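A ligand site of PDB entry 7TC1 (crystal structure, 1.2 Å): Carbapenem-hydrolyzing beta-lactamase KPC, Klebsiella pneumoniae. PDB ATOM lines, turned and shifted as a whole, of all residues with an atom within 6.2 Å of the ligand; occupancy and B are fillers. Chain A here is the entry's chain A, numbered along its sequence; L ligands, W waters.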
ATOM      1  N   LEU A  44     -14.944  17.523  -9.715  1.00  0.00           N
ATOM      2  CA  LEU A  44     -14.106  18.724  -9.783  1.00  0.00           C
ATOM      3  C   LEU A  44     -14.158  19.491  -8.466  1.00  0.00           C
ATOM      4  O   LEU A  44     -13.131  20.016  -8.003  1.00  0.00           O
ATOM      5  CB  LEU A  44     -14.551  19.605 -10.909  1.00  0.00           C
ATOM      6  CG  LEU A  44     -14.111  19.098 -12.298  1.00  0.00           C
ATOM      7  CD1 LEU A  44     -14.964  19.720 -13.392  1.00  0.00           C
ATOM      8  CD2 LEU A  44     -12.657  19.452 -12.566  1.00  0.00           C
ATOM      9  N   CYS A  45     -15.343  19.655  -7.927  1.00  0.00           N
ATOM     10  CA  CYS A  45     -15.551  20.553  -6.757  1.00  0.00           C
ATOM     11  C   CYS A  45     -14.955  21.913  -7.127  1.00  0.00           C
ATOM     12  O   CYS A  45     -14.956  22.300  -8.293  1.00  0.00           O
ATOM     13  CB  CYS A  45     -14.957  19.935  -5.492  1.00  0.00           C
ATOM     14  SG  CYS A  45     -15.281  18.160  -5.307  1.00  0.00           S
ATOM     15  N   SER A  46     -14.397  22.632  -6.133  1.00  0.00           N
ATOM     16  CA  SER A  46     -13.938  24.016  -6.356  1.00  0.00           C
ATOM     17  C   SER A  46     -12.721  24.062  -7.282  1.00  0.00           C
ATOM     18  O   SER A  46     -12.360  25.172  -7.716  1.00  0.00           O
ATOM     19  CB  SER A  46     -13.652  24.765  -5.053  1.00  0.00           C
ATOM     20  OG  SER A  46     -14.805  25.005  -4.317  1.00  0.00           O
ATOM     21  N   SER A  47     -12.133  22.945  -7.634  1.00  0.00           N
ATOM     22  CA  SER A  47     -10.992  22.988  -8.547  1.00  0.00           C
ATOM     23  C   SER A  47     -11.383  23.487  -9.915  1.00  0.00           C
ATOM     24  O   SER A  47     -10.538  23.970 -10.680  1.00  0.00           O
ATOM     25  CB  SER A  47     -10.249  21.643  -8.613  1.00  0.00           C
ATOM     26  OG  SER A  47     -10.922  20.691  -9.429  1.00  0.00           O
ATOM     27  N   LYS A  49     -12.634  26.209 -10.463  1.00  0.00           N
ATOM     28  CA  LYS A  49     -12.500  27.664 -10.455  1.00  0.00           C
ATOM     29  C   LYS A  49     -11.164  28.114 -11.047  1.00  0.00           C
ATOM     30  O   LYS A  49     -11.066  29.245 -11.504  1.00  0.00           O
ATOM     31  CB  LYS A  49     -12.688  28.209  -9.054  1.00  0.00           C
ATOM     32  CG  LYS A  49     -14.088  27.958  -8.473  1.00  0.00           C
ATOM     33  CD  LYS A  49     -14.171  28.121  -6.973  1.00  0.00           C
ATOM     34  CE  LYS A  49     -15.566  27.773  -6.483  1.00  0.00           C
ATOM     35  NZ  LYS A  49     -15.663  27.544  -5.014  1.00  0.00           N
ATOM     36  N   PRO A  80     -23.160  30.614   0.349  1.00  0.00           N
ATOM     37  CA  PRO A  80     -22.227  30.228   1.400  1.00  0.00           C
ATOM     38  C   PRO A  80     -20.791  30.100   0.873  1.00  0.00           C
ATOM     39  O   PRO A  80     -20.567  29.737  -0.273  1.00  0.00           O
ATOM     40  CB  PRO A  80     -22.787  28.882   1.873  1.00  0.00           C
ATOM     41  CG  PRO A  80     -24.301  29.069   1.646  1.00  0.00           C
ATOM     42  CD  PRO A  80     -24.337  29.719   0.290  1.00  0.00           C
ATOM     43  N   TRP A  81     -19.861  30.410   1.756  1.00  0.00           N
ATOM     44  CA  TRP A  81     -18.405  30.405   1.445  1.00  0.00           C
ATOM     45  C   TRP A  81     -18.095  31.444   0.355  1.00  0.00           C
ATOM     46  O   TRP A  81     -17.493  31.119  -0.693  1.00  0.00           O
ATOM     47  CB  TRP A  81     -17.814  29.033   1.084  1.00  0.00           C
ATOM     48  CG  TRP A  81     -16.282  29.002   1.150  1.00  0.00           C
ATOM     49  CD1 TRP A  81     -15.342  29.363   0.211  1.00  0.00           C
ATOM     50  CD2 TRP A  81     -15.537  28.496   2.264  1.00  0.00           C
ATOM     51  NE1 TRP A  81     -14.087  29.185   0.719  1.00  0.00           N
ATOM     52  CE2 TRP A  81     -14.149  28.617   1.952  1.00  0.00           C
ATOM     53  CE3 TRP A  81     -15.895  27.939   3.505  1.00  0.00           C
ATOM     54  CZ2 TRP A  81     -13.134  28.218   2.834  1.00  0.00           C
ATOM     55  CZ3 TRP A  81     -14.894  27.532   4.364  1.00  0.00           C
ATOM     56  CH2 TRP A  81     -13.545  27.647   4.026  1.00  0.00           C
ATOM     57  N   TYR A 105      -9.182  32.049  -2.774  1.00  0.00           N
ATOM     58  CA  TYR A 105     -10.047  31.829  -1.617  1.00  0.00           C
ATOM     59  C   TYR A 105     -11.166  30.856  -1.920  1.00  0.00           C
ATOM     60  O   TYR A 105     -11.962  30.551  -1.004  1.00  0.00           O
ATOM     61  CB  TYR A 105     -10.597  33.158  -1.067  1.00  0.00           C
ATOM     62  CG  TYR A 105      -9.533  34.034  -0.461  1.00  0.00           C
ATOM     63  CD1 TYR A 105      -9.123  33.862   0.853  1.00  0.00           C
ATOM     64  CD2 TYR A 105      -8.858  34.954  -1.235  1.00  0.00           C
ATOM     65  CE1 TYR A 105      -8.112  34.651   1.383  1.00  0.00           C
ATOM     66  CE2 TYR A 105      -7.820  35.710  -0.745  1.00  0.00           C
ATOM     67  CZ  TYR A 105      -7.433  35.552   0.561  1.00  0.00           C
ATOM     68  OH  TYR A 105      -6.445  36.325   1.102  1.00  0.00           O
ATOM     69  N   SER A 106     -11.303  30.406  -3.149  1.00  0.00           N
ATOM     70  CA  SER A 106     -12.416  29.509  -3.569  1.00  0.00           C
ATOM     71  C   SER A 106     -13.764  30.202  -3.386  1.00  0.00           C
ATOM     72  O   SER A 106     -14.782  29.523  -3.194  1.00  0.00           O
ATOM     73  CB  SER A 106     -12.385  28.213  -2.866  1.00  0.00           C
ATOM     74  OG  SER A 106     -11.536  27.353  -3.461  1.00  0.00           O
ATOM     75  N   ASP A 107     -13.810  31.535  -3.475  1.00  0.00           N
ATOM     76  CA  ASP A 107     -15.050  32.284  -3.206  1.00  0.00           C
ATOM     77  C   ASP A 107     -16.169  31.829  -4.148  1.00  0.00           C
ATOM     78  O   ASP A 107     -16.030  31.871  -5.388  1.00  0.00           O
ATOM     79  CB  ASP A 107     -14.746  33.756  -3.372  1.00  0.00           C
ATOM     80  CG  ASP A 107     -15.853  34.674  -2.878  1.00  0.00           C
ATOM     81  OD1 ASP A 107     -16.888  34.738  -3.590  1.00  0.00           O
ATOM     82  OD2 ASP A 107     -15.691  35.315  -1.817  1.00  0.00           O
ATOM     83  N   ASN A 108     -17.295  31.364  -3.569  1.00  0.00           N
ATOM     84  CA  ASN A 108     -18.376  30.760  -4.379  1.00  0.00           C
ATOM     85  C   ASN A 108     -19.145  31.799  -5.191  1.00  0.00           C
ATOM     86  O   ASN A 108     -19.455  31.576  -6.363  1.00  0.00           O
ATOM     87  CB  ASN A 108     -19.299  29.936  -3.509  1.00  0.00           C
ATOM     88  CG  ASN A 108     -18.809  28.543  -3.209  1.00  0.00           C
ATOM     89  OD1 ASN A 108     -18.127  27.957  -4.071  1.00  0.00           O
ATOM     90  ND2 ASN A 108     -19.177  27.965  -2.085  1.00  0.00           N
ATOM     91  N   GLU A 142     -22.368  26.904  -8.342  1.00  0.00           N
ATOM     92  CA  GLU A 142     -22.281  26.699  -6.892  1.00  0.00           C
ATOM     93  C   GLU A 142     -23.679  26.891  -6.307  1.00  0.00           C
ATOM     94  O   GLU A 142     -24.340  27.853  -6.673  1.00  0.00           O
ATOM     95  CB  GLU A 142     -21.287  27.675  -6.276  1.00  0.00           C
ATOM     96  CG  GLU A 142     -19.867  27.431  -6.658  1.00  0.00           C
ATOM     97  CD  GLU A 142     -19.294  26.188  -6.018  1.00  0.00           C
ATOM     98  OE1 GLU A 142     -19.946  25.497  -5.259  1.00  0.00           O
ATOM     99  OE2 GLU A 142     -18.085  25.914  -6.386  1.00  0.00           O
ATOM    100  N   LEU A 143     -24.128  26.060  -5.375  1.00  0.00           N
ATOM    101  CA  LEU A 143     -23.436  24.952  -4.717  1.00  0.00           C
ATOM    102  C   LEU A 143     -23.769  23.581  -5.325  1.00  0.00           C
ATOM    103  O   LEU A 143     -23.201  22.553  -4.877  1.00  0.00           O
ATOM    104  CB  LEU A 143     -23.824  24.859  -3.234  1.00  0.00           C
ATOM    105  CG  LEU A 143     -23.529  26.036  -2.371  1.00  0.00           C
ATOM    106  CD1 LEU A 143     -24.188  25.873  -1.007  1.00  0.00           C
ATOM    107  CD2 LEU A 143     -22.054  26.269  -2.246  1.00  0.00           C
ATOM    108  N   LEU A 145     -23.026  21.851  -7.919  1.00  0.00           N
ATOM    109  CA  LEU A 145     -22.011  20.997  -8.558  1.00  0.00           C
ATOM    110  C   LEU A 145     -21.268  20.127  -7.535  1.00  0.00           C
ATOM    111  O   LEU A 145     -20.453  19.278  -7.956  1.00  0.00           O
ATOM    112  CB  LEU A 145     -21.045  21.845  -9.359  1.00  0.00           C
ATOM    113  CG  LEU A 145     -20.105  22.770  -8.597  1.00  0.00           C
ATOM    114  CD1 LEU A 145     -18.708  22.293  -8.606  1.00  0.00           C
ATOM    115  CD2 LEU A 145     -20.064  24.152  -9.278  1.00  0.00           C
ATOM    116  N   ASN A 146     -21.492  20.312  -6.224  1.00  0.00           N
ATOM    117  CA  ASN A 146     -20.698  19.640  -5.171  1.00  0.00           C
ATOM    118  C   ASN A 146     -21.259  18.314  -4.687  1.00  0.00           C
ATOM    119  O   ASN A 146     -20.678  17.747  -3.762  1.00  0.00           O
ATOM    120  CB  ASN A 146     -20.551  20.586  -3.997  1.00  0.00           C
ATOM    121  CG  ASN A 146     -19.823  21.810  -4.395  1.00  0.00           C
ATOM    122  OD1 ASN A 146     -18.982  21.768  -5.255  1.00  0.00           O
ATOM    123  ND2 ASN A 146     -20.089  22.903  -3.707  1.00  0.00           N
ATOM    124  N   THR A 192      -5.493  28.499  -0.030  1.00  0.00           N
ATOM    125  CA  THR A 192      -6.297  27.371   0.461  1.00  0.00           C
ATOM    126  C   THR A 192      -5.538  26.036   0.442  1.00  0.00           C
ATOM    127  O   THR A 192      -6.113  24.989   0.857  1.00  0.00           O
ATOM    128  CB  THR A 192      -7.586  27.186  -0.353  1.00  0.00           C
ATOM    129  OG1 THR A 192      -7.191  26.746  -1.641  1.00  0.00           O
ATOM    130  CG2 THR A 192      -8.431  28.458  -0.398  1.00  0.00           C
ATOM    131  N   ARG A 196      -2.002  20.570   1.253  1.00  0.00           N
ATOM    132  CA  ARG A 196      -2.183  19.599   0.161  1.00  0.00           C
ATOM    133  C   ARG A 196      -0.879  19.473  -0.640  1.00  0.00           C
ATOM    134  O   ARG A 196       0.149  19.134  -0.031  1.00  0.00           O
ATOM    135  CB  ARG A 196      -3.431  19.960  -0.632  1.00  0.00           C
ATOM    136  CG  ARG A 196      -4.669  19.811   0.222  1.00  0.00           C
ATOM    137  CD  ARG A 196      -5.964  20.108  -0.493  1.00  0.00           C
ATOM    138  NE  ARG A 196      -7.044  20.142   0.451  1.00  0.00           N
ATOM    139  CZ  ARG A 196      -8.365  20.186   0.135  1.00  0.00           C
ATOM    140  NH1 ARG A 196      -8.776  20.091  -1.122  1.00  0.00           N
ATOM    141  NH2 ARG A 196      -9.264  20.308   1.108  1.00  0.00           N
ATOM    142  N   LYS A 210      -4.576  24.964  -7.207  1.00  0.00           N
ATOM    143  CA  LYS A 210      -5.977  25.198  -6.982  1.00  0.00           C
ATOM    144  C   LYS A 210      -6.553  23.973  -6.341  1.00  0.00           C
ATOM    145  O   LYS A 210      -6.491  22.859  -6.893  1.00  0.00           O
ATOM    146  CB  LYS A 210      -6.747  25.486  -8.267  1.00  0.00           C
ATOM    147  CG  LYS A 210      -8.225  25.734  -8.042  1.00  0.00           C
ATOM    148  CD  LYS A 210      -8.557  27.129  -7.512  1.00  0.00           C
ATOM    149  CE  LYS A 210      -9.897  27.226  -6.809  1.00  0.00           C
ATOM    150  NZ  LYS A 210      -9.860  26.600  -5.488  1.00  0.00           N
ATOM    151  N   THR A 211      -7.233  24.156  -5.186  1.00  0.00           N
ATOM    152  CA  THR A 211      -7.893  23.102  -4.420  1.00  0.00           C
ATOM    153  C   THR A 211      -9.351  22.937  -4.813  1.00  0.00           C
ATOM    154  O   THR A 211      -9.985  23.834  -5.357  1.00  0.00           O
ATOM    155  CB  THR A 211      -7.770  23.377  -2.922  1.00  0.00           C
ATOM    156  OG1 THR A 211      -8.360  24.654  -2.685  1.00  0.00           O
ATOM    157  CG2 THR A 211      -6.356  23.398  -2.400  1.00  0.00           C
ATOM    158  N   GLY A 212      -9.922  21.830  -4.336  1.00  0.00           N
ATOM    159  CA  GLY A 212     -11.371  21.694  -4.285  1.00  0.00           C
ATOM    160  C   GLY A 212     -11.779  20.809  -3.135  1.00  0.00           C
ATOM    161  O   GLY A 212     -11.099  19.808  -2.845  1.00  0.00           O
ATOM    162  N   THR A 213     -12.926  21.103  -2.551  1.00  0.00           N
ATOM    163  CA  THR A 213     -13.457  20.297  -1.455  1.00  0.00           C
ATOM    164  C   THR A 213     -14.962  20.151  -1.617  1.00  0.00           C
ATOM    165  O   THR A 213     -15.720  21.081  -1.330  1.00  0.00           O
ATOM    166  CB  THR A 213     -13.102  20.839  -0.064  1.00  0.00           C
ATOM    167  OG1 THR A 213     -11.720  21.096   0.024  1.00  0.00           O
ATOM    168  CG2 THR A 213     -13.499  19.867   1.022  1.00  0.00           C
ATOM    169  N   CYS A 214     -15.445  18.997  -2.075  1.00  0.00           N
ATOM    170  CA  CYS A 214     -16.859  18.660  -2.003  1.00  0.00           C
ATOM    171  C   CYS A 214     -17.219  18.161  -0.598  1.00  0.00           C
ATOM    172  O   CYS A 214     -18.330  18.396  -0.155  1.00  0.00           O
ATOM    173  CB  CYS A 214     -17.283  17.619  -3.031  1.00  0.00           C
ATOM    174  SG  CYS A 214     -17.284  18.091  -4.774  1.00  0.00           S
ATOM    175  N   GLY A 215     -16.282  17.497   0.059  1.00  0.00           N
ATOM    176  CA  GLY A 215     -16.435  17.079   1.481  1.00  0.00           C
ATOM    177  C   GLY A 215     -17.207  15.792   1.632  1.00  0.00           C
ATOM    178  O   GLY A 215     -16.686  14.795   2.150  1.00  0.00           O
ATOM    179  N   ASN A 221      -9.532  17.555  -3.595  1.00  0.00           N
ATOM    180  CA  ASN A 221      -8.512  17.488  -4.655  1.00  0.00           C
ATOM    181  C   ASN A 221      -7.619  18.694  -4.620  1.00  0.00           C
ATOM    182  O   ASN A 221      -7.840  19.658  -3.864  1.00  0.00           O
ATOM    183  CB  ASN A 221      -9.217  17.292  -6.014  1.00  0.00           C
ATOM    184  CG  ASN A 221     -10.267  18.343  -6.237  1.00  0.00           C
ATOM    185  OD1 ASN A 221      -9.947  19.522  -6.233  1.00  0.00           O
ATOM    186  ND2 ASN A 221     -11.525  17.924  -6.400  1.00  0.00           N
ATOM    187  N   HIS A 249     -13.037  13.501   3.669  1.00  0.00           N
ATOM    188  CA  HIS A 249     -11.849  13.769   2.875  1.00  0.00           C
ATOM    189  C   HIS A 249     -10.664  13.935   3.813  1.00  0.00           C
ATOM    190  O   HIS A 249     -10.820  14.122   5.029  1.00  0.00           O
ATOM    191  CB  HIS A 249     -12.009  14.994   1.965  1.00  0.00           C
ATOM    192  CG  HIS A 249     -11.848  16.299   2.660  1.00  0.00           C
ATOM    193  ND1 HIS A 249     -12.872  16.907   3.372  1.00  0.00           N
ATOM    194  CD2 HIS A 249     -10.806  17.160   2.702  1.00  0.00           C
ATOM    195  CE1 HIS A 249     -12.407  18.042   3.873  1.00  0.00           C
ATOM    196  NE2 HIS A 249     -11.158  18.220   3.464  1.00  0.00           N
HETATM  197  C1  LIG L   1     -15.512  24.248   3.096  1.00  0.00           C
HETATM  198  C2  LIG L   1     -17.157  23.447   1.437  1.00  0.00           C
HETATM  199  C3  LIG L   1     -15.384  22.935   2.865  1.00  0.00           C
HETATM  200  C4  LIG L   1     -18.127  24.265  -0.694  1.00  0.00           C
HETATM  201  C5  LIG L   1     -15.909  26.119  -1.581  1.00  0.00           C
HETATM  202  C6  LIG L   1     -14.745  25.734  -0.711  1.00  0.00           C
HETATM  203  C7  LIG L   1     -13.633  25.099  -1.530  1.00  0.00           C
HETATM  204  C8  LIG L   1     -12.469  24.701  -0.654  1.00  0.00           C
HETATM  205  O1  LIG L   1     -10.690  23.175  -1.178  1.00  0.00           O
HETATM  206  C9  LIG L   1     -11.273  24.255  -1.460  1.00  0.00           C
HETATM  207  O2  LIG L   1     -10.852  25.015  -2.385  1.00  0.00           O
HETATM  208  O3  LIG L   1     -14.085  23.936  -2.256  1.00  0.00           O
HETATM  209  B1  LIG L   1     -15.233  24.161  -3.160  1.00  0.00           B
HETATM  210  O4  LIG L   1     -15.571  22.825  -3.663  1.00  0.00           O
HETATM  211  C10 LIG L   1     -16.410  24.910  -2.374  1.00  0.00           C
HETATM  212  N1  LIG L   1     -17.071  23.990  -1.462  1.00  0.00           N
HETATM  213  O5  LIG L   1     -18.859  25.260  -0.836  1.00  0.00           O
HETATM  214  C11 LIG L   1     -18.308  23.316   0.457  1.00  0.00           C
HETATM  215  S1  LIG L   1     -16.838  24.897   2.262  1.00  0.00           S
HETATM  216  C12 LIG L   1     -16.238  22.462   1.816  1.00  0.00           C
HETATM  217  O   HOH W   1      -8.628  23.549   0.799  1.00  0.00           O
HETATM  218  O   HOH W   2     -17.270  23.634  -5.735  1.00  0.00           O
HETATM  219  O   HOH W   3     -20.618  25.789   1.555  1.00  0.00           O
HETATM  220  O   HOH W   4     -20.094  20.476  -0.196  1.00  0.00           O
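The side-chain hydroxyl (OG1) of Thr 211 is in hydrogen-bond range of the side-chain hydroxyl (OG1) of Thr 192, at 2.6 Å.
The backbone carbonyl oxygen (O) of Thr 211 sits at hydrogen-bond distance from the backbone NH (N) of Ser 47, 3.3 Å away.
The side-chain hydroxyl (OG) of Ser 106 is in hydrogen-bond range of the side-chain amino group (NZ) of Lys 210 (2.7 Å).
O of Ser 106 is in hydrogen-bond range of NZ of Lys 49 (2.8 Å).
NZ of Lys 49 sits at hydrogen-bond distance from OD1 of Asn 108.
The side-chain amide oxygen (OD1) of Asn 108 lies close to the side-chain carboxylate (OE2) of Glu 142 (3.1 Å).
NH1 of Arg 196 sits at hydrogen-bond distance from O of Gly 212 (2.9 Å).
NH1 of Arg 196 lies within hydrogen-bond range of O of Asn 221 (2.9 Å).
Merely in contact with the ligand: Cys 45, Lys 49, Trp 81, Leu 143, Asn 146 and Gly 212.
Hydrophobic or aromatic side chains that line the ligand: Trp 81 and Leu 143.
Of the 25 residues printed, 13 come within 4 Å of the ligand.
The nearest printed residue that does not touch the ligand is Thr 192 (4.1 Å).
Water W2 lies within hydrogen-bond range of the side-chain carboxylate (OE2) of Glu 142 (2.5 Å), the side-chain amide oxygen (OD1) of Asn 146 (2.6 Å), an oxygen (O4) of the ligand (2.8 Å) and the backbone NH (N) of Ser 46 (3.1 Å).
Water W1 lies within hydrogen-bond range of an oxygen (O1) of the ligand (2.9 Å), the backbone carbonyl oxygen of Thr 192 (2.9 Å) and the guanidinium group of Arg 196 (3.3 Å).
O4 of the ligand lies within hydrogen-bond range of N of Ser 46, 2.7 Å away.
The side-chain hydroxyl (OG) of Ser 46 is bonded to a boron (B1) of the ligand (1.5 Å).
OG1 of Thr 211 sits at hydrogen-bond distance from O2 of the ligand (2.5 Å).
The backbone NH (N) of Thr 213 sits at hydrogen-bond distance from an oxygen (O3) of the ligand (3.1 Å).
O of Thr 213 lies within hydrogen-bond range of O4 of the ligand.
OG1 of Thr 213 is in hydrogen-bond range of O1 of the ligand (2.6 Å).
An oxygen (O2) of the ligand sits at hydrogen-bond distance from the side-chain hydroxyl of Ser 106, at 2.7 Å.
ND2 of Asn 108 lies within hydrogen-bond range of O5 of the ligand (3.0 Å).
The side-chain amino group (NZ) of Lys 210 is in salt-bridge range of an oxygen (O2) of the ligand.
The guanidinium group (NH1) of Arg 196 is in salt-bridge range of an oxygen (O1) of the ligand (3.6 Å).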
